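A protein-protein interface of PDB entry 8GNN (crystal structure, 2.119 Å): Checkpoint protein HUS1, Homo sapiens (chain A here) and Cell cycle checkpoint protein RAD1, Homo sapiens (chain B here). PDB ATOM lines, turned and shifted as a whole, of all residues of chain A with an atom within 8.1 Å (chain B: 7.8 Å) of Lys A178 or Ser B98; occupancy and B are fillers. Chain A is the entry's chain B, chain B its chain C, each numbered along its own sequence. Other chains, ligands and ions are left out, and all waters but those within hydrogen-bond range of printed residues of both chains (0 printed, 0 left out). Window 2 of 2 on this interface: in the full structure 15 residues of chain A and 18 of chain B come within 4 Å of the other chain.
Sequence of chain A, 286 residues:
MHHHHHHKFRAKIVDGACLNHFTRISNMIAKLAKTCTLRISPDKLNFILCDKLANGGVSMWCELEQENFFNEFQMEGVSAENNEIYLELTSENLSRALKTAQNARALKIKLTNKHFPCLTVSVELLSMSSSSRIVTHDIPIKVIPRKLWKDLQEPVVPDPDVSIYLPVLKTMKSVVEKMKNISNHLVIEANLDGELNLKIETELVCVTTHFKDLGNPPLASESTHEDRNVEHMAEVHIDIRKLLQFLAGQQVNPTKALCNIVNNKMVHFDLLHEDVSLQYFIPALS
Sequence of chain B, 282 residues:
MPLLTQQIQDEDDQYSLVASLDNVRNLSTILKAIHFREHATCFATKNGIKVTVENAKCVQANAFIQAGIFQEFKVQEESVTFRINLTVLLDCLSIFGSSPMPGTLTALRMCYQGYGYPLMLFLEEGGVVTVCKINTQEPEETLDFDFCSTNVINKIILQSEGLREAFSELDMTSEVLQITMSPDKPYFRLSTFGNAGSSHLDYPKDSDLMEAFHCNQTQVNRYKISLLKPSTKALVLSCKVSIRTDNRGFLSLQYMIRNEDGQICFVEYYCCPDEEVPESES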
ATOM      1  N   MET A 172      17.545 -34.044   8.425  1.00  0.00           N
ATOM      2  CA  MET A 172      16.296 -33.569   7.834  1.00  0.00           C
ATOM      3  C   MET A 172      15.196 -33.457   8.880  1.00  0.00           C
ATOM      4  O   MET A 172      14.478 -32.460   8.932  1.00  0.00           O
ATOM      5  CB  MET A 172      15.836 -34.499   6.710  1.00  0.00           C
ATOM      6  CG  MET A 172      16.567 -34.309   5.398  1.00  0.00           C
ATOM      7  SD  MET A 172      15.698 -35.095   4.029  1.00  0.00           S
ATOM      8  CE  MET A 172      14.244 -34.056   3.916  1.00  0.00           C
ATOM      9  N   LYS A 173      15.072 -34.491   9.706  1.00  0.00           N
ATOM     10  CA  LYS A 173      14.046 -34.534  10.741  1.00  0.00           C
ATOM     11  C   LYS A 173      14.172 -33.361  11.706  1.00  0.00           C
ATOM     12  O   LYS A 173      13.181 -32.707  12.032  1.00  0.00           O
ATOM     13  CB  LYS A 173      14.121 -35.851  11.512  1.00  0.00           C
ATOM     14  CG  LYS A 173      13.060 -35.988  12.589  1.00  0.00           C
ATOM     15  CD  LYS A 173      13.260 -37.247  13.412  1.00  0.00           C
ATOM     16  CE  LYS A 173      12.214 -37.348  14.509  1.00  0.00           C
ATOM     17  NZ  LYS A 173      12.138 -36.097  15.314  1.00  0.00           N
ATOM     18  N   SER A 174      15.397 -33.098  12.152  1.00  0.00           N
ATOM     19  CA  SER A 174      15.661 -32.014  13.092  1.00  0.00           C
ATOM     20  C   SER A 174      15.277 -30.660  12.505  1.00  0.00           C
ATOM     21  O   SER A 174      14.668 -29.830  13.180  1.00  0.00           O
ATOM     22  CB  SER A 174      17.136 -32.007  13.500  1.00  0.00           C
ATOM     23  OG  SER A 174      17.501 -33.231  14.116  1.00  0.00           O
ATOM     24  N   VAL A 175      15.635 -30.446  11.244  1.00  0.00           N
ATOM     25  CA  VAL A 175      15.326 -29.196  10.562  1.00  0.00           C
ATOM     26  C   VAL A 175      13.824 -29.046  10.341  1.00  0.00           C
ATOM     27  O   VAL A 175      13.248 -27.994  10.618  1.00  0.00           O
ATOM     28  CB  VAL A 175      16.054 -29.102   9.206  1.00  0.00           C
ATOM     29  CG1 VAL A 175      15.601 -27.869   8.441  1.00  0.00           C
ATOM     30  CG2 VAL A 175      17.562 -29.079   9.413  1.00  0.00           C
ATOM     31  N   VAL A 176      13.195 -30.110   9.853  1.00  0.00           N
ATOM     32  CA  VAL A 176      11.771 -30.091   9.533  1.00  0.00           C
ATOM     33  C   VAL A 176      10.897 -29.862  10.767  1.00  0.00           C
ATOM     34  O   VAL A 176       9.973 -29.048  10.735  1.00  0.00           O
ATOM     35  CB  VAL A 176      11.344 -31.403   8.835  1.00  0.00           C
ATOM     36  CG1 VAL A 176       9.831 -31.557   8.845  1.00  0.00           C
ATOM     37  CG2 VAL A 176      11.876 -31.440   7.408  1.00  0.00           C
ATOM     38  N   GLU A 177      11.195 -30.566  11.855  1.00  0.00           N
ATOM     39  CA  GLU A 177      10.368 -30.478  13.056  1.00  0.00           C
ATOM     40  C   GLU A 177      10.466 -29.101  13.712  1.00  0.00           C
ATOM     41  O   GLU A 177       9.525 -28.652  14.365  1.00  0.00           O
ATOM     42  CB  GLU A 177      10.750 -31.572  14.059  1.00  0.00           C
ATOM     43  CG  GLU A 177      12.060 -31.348  14.793  1.00  0.00           C
ATOM     44  CD  GLU A 177      12.378 -32.471  15.761  1.00  0.00           C
ATOM     45  OE1 GLU A 177      11.491 -33.320  15.997  1.00  0.00           O
ATOM     46  OE2 GLU A 177      13.508 -32.503  16.289  1.00  0.00           O
ATOM     47  N   LYS A 178      11.599 -28.431  13.530  1.00  0.00           N
ATOM     48  CA  LYS A 178      11.755 -27.070  14.028  1.00  0.00           C
ATOM     49  C   LYS A 178      11.060 -26.095  13.087  1.00  0.00           C
ATOM     50  O   LYS A 178      10.529 -25.070  13.518  1.00  0.00           O
ATOM     51  CB  LYS A 178      13.233 -26.708  14.182  1.00  0.00           C
ATOM     52  CG  LYS A 178      13.678 -26.510  15.624  1.00  0.00           C
ATOM     53  CD  LYS A 178      13.795 -27.834  16.361  1.00  0.00           C
ATOM     54  CE  LYS A 178      14.222 -27.625  17.806  1.00  0.00           C
ATOM     55  NZ  LYS A 178      14.337 -28.911  18.547  1.00  0.00           N
ATOM     56  N   MET A 179      11.062 -26.421  11.797  1.00  0.00           N
ATOM     57  CA  MET A 179      10.352 -25.619  10.807  1.00  0.00           C
ATOM     58  C   MET A 179       8.846 -25.738  11.007  1.00  0.00           C
ATOM     59  O   MET A 179       8.094 -24.816  10.691  1.00  0.00           O
ATOM     60  CB  MET A 179      10.735 -26.042   9.385  1.00  0.00           C
ATOM     61  CG  MET A 179      12.084 -25.513   8.919  1.00  0.00           C
ATOM     62  SD  MET A 179      12.355 -25.723   7.146  1.00  0.00           S
ATOM     63  CE  MET A 179      12.282 -27.504   6.990  1.00  0.00           C
ATOM     64  N   LYS A 180       8.412 -26.878  11.538  1.00  0.00           N
ATOM     65  CA  LYS A 180       6.999 -27.109  11.821  1.00  0.00           C
ATOM     66  C   LYS A 180       6.485 -26.128  12.871  1.00  0.00           C
ATOM     67  O   LYS A 180       5.318 -25.736  12.848  1.00  0.00           O
ATOM     68  CB  LYS A 180       6.770 -28.547  12.291  1.00  0.00           C
ATOM     69  CG  LYS A 180       5.305 -28.893  12.518  1.00  0.00           C
ATOM     70  CD  LYS A 180       5.147 -30.213  13.251  1.00  0.00           C
ATOM     71  CE  LYS A 180       3.684 -30.620  13.340  1.00  0.00           C
ATOM     72  NZ  LYS A 180       2.844 -29.547  13.943  1.00  0.00           N
ATOM     73  N   ASN A 181       7.364 -25.733  13.787  1.00  0.00           N
ATOM     74  CA  ASN A 181       7.013 -24.767  14.823  1.00  0.00           C
ATOM     75  C   ASN A 181       6.710 -23.392  14.238  1.00  0.00           C
ATOM     76  O   ASN A 181       6.050 -22.569  14.871  1.00  0.00           O
ATOM     77  CB  ASN A 181       8.142 -24.648  15.851  1.00  0.00           C
ATOM     78  CG  ASN A 181       8.444 -25.963  16.541  1.00  0.00           C
ATOM     79  OD1 ASN A 181       7.596 -26.853  16.606  1.00  0.00           O
ATOM     80  ND2 ASN A 181       9.658 -26.092  17.063  1.00  0.00           N
ATOM     81  N   ILE A 182       7.197 -23.153  13.025  1.00  0.00           N
ATOM     82  CA  ILE A 182       7.049 -21.855  12.378  1.00  0.00           C
ATOM     83  C   ILE A 182       5.897 -21.842  11.377  1.00  0.00           C
ATOM     84  O   ILE A 182       5.036 -20.963  11.422  1.00  0.00           O
ATOM     85  CB  ILE A 182       8.345 -21.448  11.660  1.00  0.00           C
ATOM     86  CG1 ILE A 182       9.479 -21.277  12.674  1.00  0.00           C
ATOM     87  CG2 ILE A 182       8.137 -20.169  10.867  1.00  0.00           C
ATOM     88  CD1 ILE A 182      10.809 -20.918  12.051  1.00  0.00           C
ATOM     89  N   SER A 183       5.886 -22.818  10.475  1.00  0.00           N
ATOM     90  CA  SER A 183       4.838 -22.910   9.467  1.00  0.00           C
ATOM     91  C   SER A 183       4.424 -24.357   9.228  1.00  0.00           C
ATOM     92  O   SER A 183       5.104 -25.288   9.657  1.00  0.00           O
ATOM     93  CB  SER A 183       5.299 -22.275   8.154  1.00  0.00           C
ATOM     94  OG  SER A 183       4.288 -22.354   7.165  1.00  0.00           O
ATOM     95  N   ILE A 200      10.473 -22.807   4.129  1.00  0.00           N
ATOM     96  CA  ILE A 200       9.218 -22.319   4.682  1.00  0.00           C
ATOM     97  C   ILE A 200       9.236 -20.797   4.612  1.00  0.00           C
ATOM     98  O   ILE A 200      10.299 -20.176   4.673  1.00  0.00           O
ATOM     99  CB  ILE A 200       8.990 -22.783   6.135  1.00  0.00           C
ATOM    100  CG1 ILE A 200      10.069 -22.222   7.061  1.00  0.00           C
ATOM    101  CG2 ILE A 200       8.950 -24.301   6.211  1.00  0.00           C
ATOM    102  CD1 ILE A 200       9.863 -22.573   8.515  1.00  0.00           C
ATOM    103  N   VAL A 207      12.707 -19.165   6.124  1.00  0.00           N
ATOM    104  CA  VAL A 207      13.767 -20.098   6.487  1.00  0.00           C
ATOM    105  C   VAL A 207      14.084 -21.044   5.335  1.00  0.00           C
ATOM    106  O   VAL A 207      13.198 -21.716   4.808  1.00  0.00           O
ATOM    107  CB  VAL A 207      13.398 -20.931   7.732  1.00  0.00           C
ATOM    108  CG1 VAL A 207      14.514 -21.910   8.064  1.00  0.00           C
ATOM    109  CG2 VAL A 207      13.116 -20.024   8.918  1.00  0.00           C
ATOM    110  N   ILE A 240       3.996 -30.139   5.732  1.00  0.00           N
ATOM    111  CA  ILE A 240       5.241 -30.439   6.434  1.00  0.00           C
ATOM    112  C   ILE A 240       5.069 -31.531   7.490  1.00  0.00           C
ATOM    113  O   ILE A 240       6.025 -32.223   7.841  1.00  0.00           O
ATOM    114  CB  ILE A 240       5.825 -29.165   7.098  1.00  0.00           C
ATOM    115  CG1 ILE A 240       7.299 -29.366   7.457  1.00  0.00           C
ATOM    116  CG2 ILE A 240       5.010 -28.759   8.320  1.00  0.00           C
ATOM    117  CD1 ILE A 240       7.947 -28.151   8.083  1.00  0.00           C
ATOM    118  N   LEU A 244       7.372 -34.813   8.087  1.00  0.00           N
ATOM    119  CA  LEU A 244       7.866 -35.085   9.430  1.00  0.00           C
ATOM    120  C   LEU A 244       7.437 -36.473   9.890  1.00  0.00           C
ATOM    121  O   LEU A 244       8.205 -37.187  10.536  1.00  0.00           O
ATOM    122  CB  LEU A 244       7.370 -34.024  10.414  1.00  0.00           C
ATOM    123  CG  LEU A 244       7.875 -34.165  11.851  1.00  0.00           C
ATOM    124  CD1 LEU A 244       9.395 -34.249  11.879  1.00  0.00           C
ATOM    125  CD2 LEU A 244       7.383 -33.011  12.707  1.00  0.00           C
ATOM    126  N   ARG B  25      25.010 -22.528  20.574  1.00  0.00           N
ATOM    127  CA  ARG B  25      24.419 -22.789  21.881  1.00  0.00           C
ATOM    128  C   ARG B  25      24.877 -21.777  22.931  1.00  0.00           C
ATOM    129  O   ARG B  25      24.219 -21.601  23.953  1.00  0.00           O
ATOM    130  CB  ARG B  25      24.742 -24.213  22.339  1.00  0.00           C
ATOM    131  CG  ARG B  25      24.149 -25.290  21.438  1.00  0.00           C
ATOM    132  CD  ARG B  25      24.167 -26.660  22.098  1.00  0.00           C
ATOM    133  NE  ARG B  25      25.518 -27.106  22.423  1.00  0.00           N
ATOM    134  CZ  ARG B  25      26.297 -27.794  21.595  1.00  0.00           C
ATOM    135  NH1 ARG B  25      25.861 -28.115  20.384  1.00  0.00           N
ATOM    136  NH2 ARG B  25      27.513 -28.161  21.974  1.00  0.00           N
ATOM    137  N   SER B  28      21.913 -19.416  22.246  1.00  0.00           N
ATOM    138  CA  SER B  28      20.566 -19.965  22.356  1.00  0.00           C
ATOM    139  C   SER B  28      20.245 -20.443  23.770  1.00  0.00           C
ATOM    140  O   SER B  28      19.131 -20.246  24.255  1.00  0.00           O
ATOM    141  CB  SER B  28      20.374 -21.113  21.363  1.00  0.00           C
ATOM    142  OG  SER B  28      21.255 -22.185  21.642  1.00  0.00           O
ATOM    143  N   THR B  29      21.219 -21.066  24.428  1.00  0.00           N
ATOM    144  CA  THR B  29      21.007 -21.627  25.761  1.00  0.00           C
ATOM    145  C   THR B  29      20.631 -20.555  26.779  1.00  0.00           C
ATOM    146  O   THR B  29      19.701 -20.734  27.565  1.00  0.00           O
ATOM    147  CB  THR B  29      22.257 -22.376  26.264  1.00  0.00           C
ATOM    148  OG1 THR B  29      22.574 -23.442  25.360  1.00  0.00           O
ATOM    149  CG2 THR B  29      22.018 -22.951  27.651  1.00  0.00           C
ATOM    150  N   LYS B  32      17.100 -19.018  26.193  1.00  0.00           N
ATOM    151  CA  LYS B  32      16.004 -19.876  26.634  1.00  0.00           C
ATOM    152  C   LYS B  32      15.634 -19.610  28.091  1.00  0.00           C
ATOM    153  O   LYS B  32      14.508 -19.870  28.513  1.00  0.00           O
ATOM    154  CB  LYS B  32      16.368 -21.353  26.451  1.00  0.00           C
ATOM    155  CG  LYS B  32      16.469 -21.801  25.002  1.00  0.00           C
ATOM    156  CD  LYS B  32      16.935 -23.247  24.900  1.00  0.00           C
ATOM    157  CE  LYS B  32      17.048 -23.689  23.449  1.00  0.00           C
ATOM    158  NZ  LYS B  32      17.494 -25.106  23.330  1.00  0.00           N
ATOM    159  N   THR B  87      10.478 -16.448  20.138  1.00  0.00           N
ATOM    160  CA  THR B  87      10.135 -17.840  19.869  1.00  0.00           C
ATOM    161  C   THR B  87      10.657 -18.278  18.504  1.00  0.00           C
ATOM    162  O   THR B  87      11.229 -19.359  18.367  1.00  0.00           O
ATOM    163  CB  THR B  87       8.613 -18.067  19.929  1.00  0.00           C
ATOM    164  OG1 THR B  87       8.102 -17.580  21.176  1.00  0.00           O
ATOM    165  CG2 THR B  87       8.290 -19.549  19.797  1.00  0.00           C
ATOM    166  N   VAL B  88      10.463 -17.428  17.499  1.00  0.00           N
ATOM    167  CA  VAL B  88      10.954 -17.707  16.154  1.00  0.00           C
ATOM    168  C   VAL B  88      12.479 -17.704  16.128  1.00  0.00           C
ATOM    169  O   VAL B  88      13.100 -18.565  15.501  1.00  0.00           O
ATOM    170  CB  VAL B  88      10.415 -16.684  15.131  1.00  0.00           C
ATOM    171  CG1 VAL B  88      11.081 -16.875  13.776  1.00  0.00           C
ATOM    172  CG2 VAL B  88       8.905 -16.804  15.006  1.00  0.00           C
ATOM    173  N   LEU B  90      14.542 -18.410  18.579  1.00  0.00           N
ATOM    174  CA  LEU B  90      15.024 -19.621  19.234  1.00  0.00           C
ATOM    175  C   LEU B  90      14.774 -20.871  18.391  1.00  0.00           C
ATOM    176  O   LEU B  90      15.569 -21.810  18.419  1.00  0.00           O
ATOM    177  CB  LEU B  90      14.375 -19.773  20.610  1.00  0.00           C
ATOM    178  CG  LEU B  90      14.927 -18.835  21.686  1.00  0.00           C
ATOM    179  CD1 LEU B  90      14.069 -18.876  22.939  1.00  0.00           C
ATOM    180  CD2 LEU B  90      16.369 -19.194  22.010  1.00  0.00           C
ATOM    181  N   ASP B  91      13.673 -20.880  17.646  1.00  0.00           N
ATOM    182  CA  ASP B  91      13.398 -21.974  16.719  1.00  0.00           C
ATOM    183  C   ASP B  91      14.473 -22.033  15.639  1.00  0.00           C
ATOM    184  O   ASP B  91      14.924 -23.112  15.253  1.00  0.00           O
ATOM    185  CB  ASP B  91      12.016 -21.818  16.077  1.00  0.00           C
ATOM    186  CG  ASP B  91      10.898 -22.328  16.966  1.00  0.00           C
ATOM    187  OD1 ASP B  91      11.115 -23.329  17.682  1.00  0.00           O
ATOM    188  OD2 ASP B  91       9.801 -21.733  16.942  1.00  0.00           O
ATOM    189  N   CYS B  92      14.883 -20.861  15.164  1.00  0.00           N
ATOM    190  CA  CYS B  92      15.896 -20.764  14.120  1.00  0.00           C
ATOM    191  C   CYS B  92      17.288 -21.107  14.641  1.00  0.00           C
ATOM    192  O   CYS B  92      18.055 -21.795  13.970  1.00  0.00           O
ATOM    193  CB  CYS B  92      15.902 -19.359  13.513  1.00  0.00           C
ATOM    194  SG  CYS B  92      14.398 -18.932  12.607  1.00  0.00           S
ATOM    195  N   LEU B  93      17.612 -20.625  15.837  1.00  0.00           N
ATOM    196  CA  LEU B  93      18.926 -20.869  16.426  1.00  0.00           C
ATOM    197  C   LEU B  93      19.146 -22.350  16.722  1.00  0.00           C
ATOM    198  O   LEU B  93      20.282 -22.821  16.762  1.00  0.00           O
ATOM    199  CB  LEU B  93      19.101 -20.047  17.706  1.00  0.00           C
ATOM    200  CG  LEU B  93      19.207 -18.531  17.526  1.00  0.00           C
ATOM    201  CD1 LEU B  93      19.362 -17.837  18.872  1.00  0.00           C
ATOM    202  CD2 LEU B  93      20.360 -18.180  16.598  1.00  0.00           C
ATOM    203  N   SER B  94      18.053 -23.079  16.925  1.00  0.00           N
ATOM    204  CA  SER B  94      18.127 -24.508  17.203  1.00  0.00           C
ATOM    205  C   SER B  94      17.568 -25.328  16.044  1.00  0.00           C
ATOM    206  O   SER B  94      17.037 -26.420  16.244  1.00  0.00           O
ATOM    207  CB  SER B  94      17.371 -24.839  18.491  1.00  0.00           C
ATOM    208  OG  SER B  94      16.010 -24.460  18.389  1.00  0.00           O
ATOM    209  N   ILE B  95      17.703 -24.797  14.832  1.00  0.00           N
ATOM    210  CA  ILE B  95      17.129 -25.421  13.642  1.00  0.00           C
ATOM    211  C   ILE B  95      17.747 -26.791  13.347  1.00  0.00           C
ATOM    212  O   ILE B  95      17.114 -27.640  12.719  1.00  0.00           O
ATOM    213  CB  ILE B  95      17.289 -24.503  12.401  1.00  0.00           C
ATOM    214  CG1 ILE B  95      16.429 -24.996  11.233  1.00  0.00           C
ATOM    215  CG2 ILE B  95      18.753 -24.374  11.999  1.00  0.00           C
ATOM    216  CD1 ILE B  95      14.941 -24.913  11.490  1.00  0.00           C
ATOM    217  N   PHE B  96      18.970 -27.017  13.817  1.00  0.00           N
ATOM    218  CA  PHE B  96      19.656 -28.278  13.551  1.00  0.00           C
ATOM    219  C   PHE B  96      19.542 -29.268  14.708  1.00  0.00           C
ATOM    220  O   PHE B  96      20.299 -30.237  14.779  1.00  0.00           O
ATOM    221  CB  PHE B  96      21.132 -28.028  13.229  1.00  0.00           C
ATOM    222  CG  PHE B  96      21.366 -27.451  11.862  1.00  0.00           C
ATOM    223  CD1 PHE B  96      21.133 -28.211  10.728  1.00  0.00           C
ATOM    224  CD2 PHE B  96      21.827 -26.154  11.711  1.00  0.00           C
ATOM    225  CE1 PHE B  96      21.347 -27.686   9.467  1.00  0.00           C
ATOM    226  CE2 PHE B  96      22.046 -25.623  10.452  1.00  0.00           C
ATOM    227  CZ  PHE B  96      21.807 -26.391   9.329  1.00  0.00           C
ATOM    228  N   GLY B  97      18.595 -29.028  15.609  1.00  0.00           N
ATOM    229  CA  GLY B  97      18.363 -29.935  16.720  1.00  0.00           C
ATOM    230  C   GLY B  97      18.767 -29.352  18.060  1.00  0.00           C
ATOM    231  O   GLY B  97      19.605 -28.455  18.131  1.00  0.00           O
ATOM    232  N   SER B  98      18.173 -29.875  19.130  1.00  0.00           N
ATOM    233  CA  SER B  98      18.418 -29.358  20.472  1.00  0.00           C
ATOM    234  C   SER B  98      19.337 -30.261  21.293  1.00  0.00           C
ATOM    235  O   SER B  98      19.593 -29.988  22.465  1.00  0.00           O
ATOM    236  CB  SER B  98      17.093 -29.162  21.212  1.00  0.00           C
ATOM    237  OG  SER B  98      16.334 -28.116  20.630  1.00  0.00           O
ATOM    238  N   SER B  99      19.830 -31.333  20.681  1.00  0.00           N
ATOM    239  CA  SER B  99      20.741 -32.243  21.371  1.00  0.00           C
ATOM    240  C   SER B  99      21.711 -32.933  20.413  1.00  0.00           C
ATOM    241  O   SER B  99      21.523 -34.100  20.068  1.00  0.00           O
ATOM    242  CB  SER B  99      19.951 -33.295  22.153  1.00  0.00           C
ATOM    243  OG  SER B  99      19.273 -32.712  23.254  1.00  0.00           O
ATOM    244  N   PRO B 100      22.757 -32.210  19.982  1.00  0.00           N
ATOM    245  CA  PRO B 100      23.786 -32.774  19.101  1.00  0.00           C
ATOM    246  C   PRO B 100      24.668 -33.791  19.819  1.00  0.00           C
ATOM    247  O   PRO B 100      25.816 -33.472  20.131  1.00  0.00           O
ATOM    248  CB  PRO B 100      24.607 -31.546  18.681  1.00  0.00           C
ATOM    249  CG  PRO B 100      23.742 -30.363  19.003  1.00  0.00           C
ATOM    250  CD  PRO B 100      22.965 -30.771  20.210  1.00  0.00           C
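The backbone NH (N) of Val A175 lies close to the backbone carbonyl oxygen (O) of Ile B95 (3.5 Å). The side-chain hydroxyl of Ser B98 is in hydrogen-bond range of the side-chain amino group of Lys A178, at 3.0 Å. The side-chain amide nitrogen (ND2) of Asn A181 sits at hydrogen-bond distance from the side-chain carboxylate (OD1) of Asp B91 (3.2 Å). The backbone carbonyl oxygen (O) of Ser A174 lies close to the backbone carbonyl oxygen (O) of Ile B95, 3.3 Å away.
OD1 of Asn A181 lies close to O of Glu A177, at 3.5 Å. O of Leu B90 lies within hydrogen-bond range of OG of Ser B94 (2.7 Å).
Among the printed residues, merely in contact across the chains: Lys A178 with Ser B94, Lys A178 with Asp B91, Lys A178 with Ile B95, Ser A174 with Phe B96, Met A179 with Ile B95, Val A175 with Phe B96 and Ser A174 with Gly B97.
Of the printed residues of chain B, Ser A174 touches Ile B95 (3.3 Å), Phe B96 (3.8 Å) and Gly B97 (3.9 Å). Printed residues of chain B within 4 Å of Val A175: Ile B95 and Phe B96. Of chain B, only Asp B91, Ser B94, Ile B95 and Ser B98 come within 4 Å of Lys A178. Of the printed residues of chain A, Asp B91 touches Lys A178 and Asn A181. Of the printed residues of chain A, Gly B97 touches Ser A174. The nearest printed residue of chain A that does not touch Phe B96 is Lys A178 (5.6 Å).
Of the 16 printed residues of chain A, 5 touch a printed residue of chain B. Printed residues of chain B that touch a printed residue of chain A: Asp B91, Ser B94, Ile B95, Phe B96, Gly B97 and Ser B98. Hydrophobic or aromatic side chains of chain B that line the printed part of chain A: Ile B95 and Phe B96.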
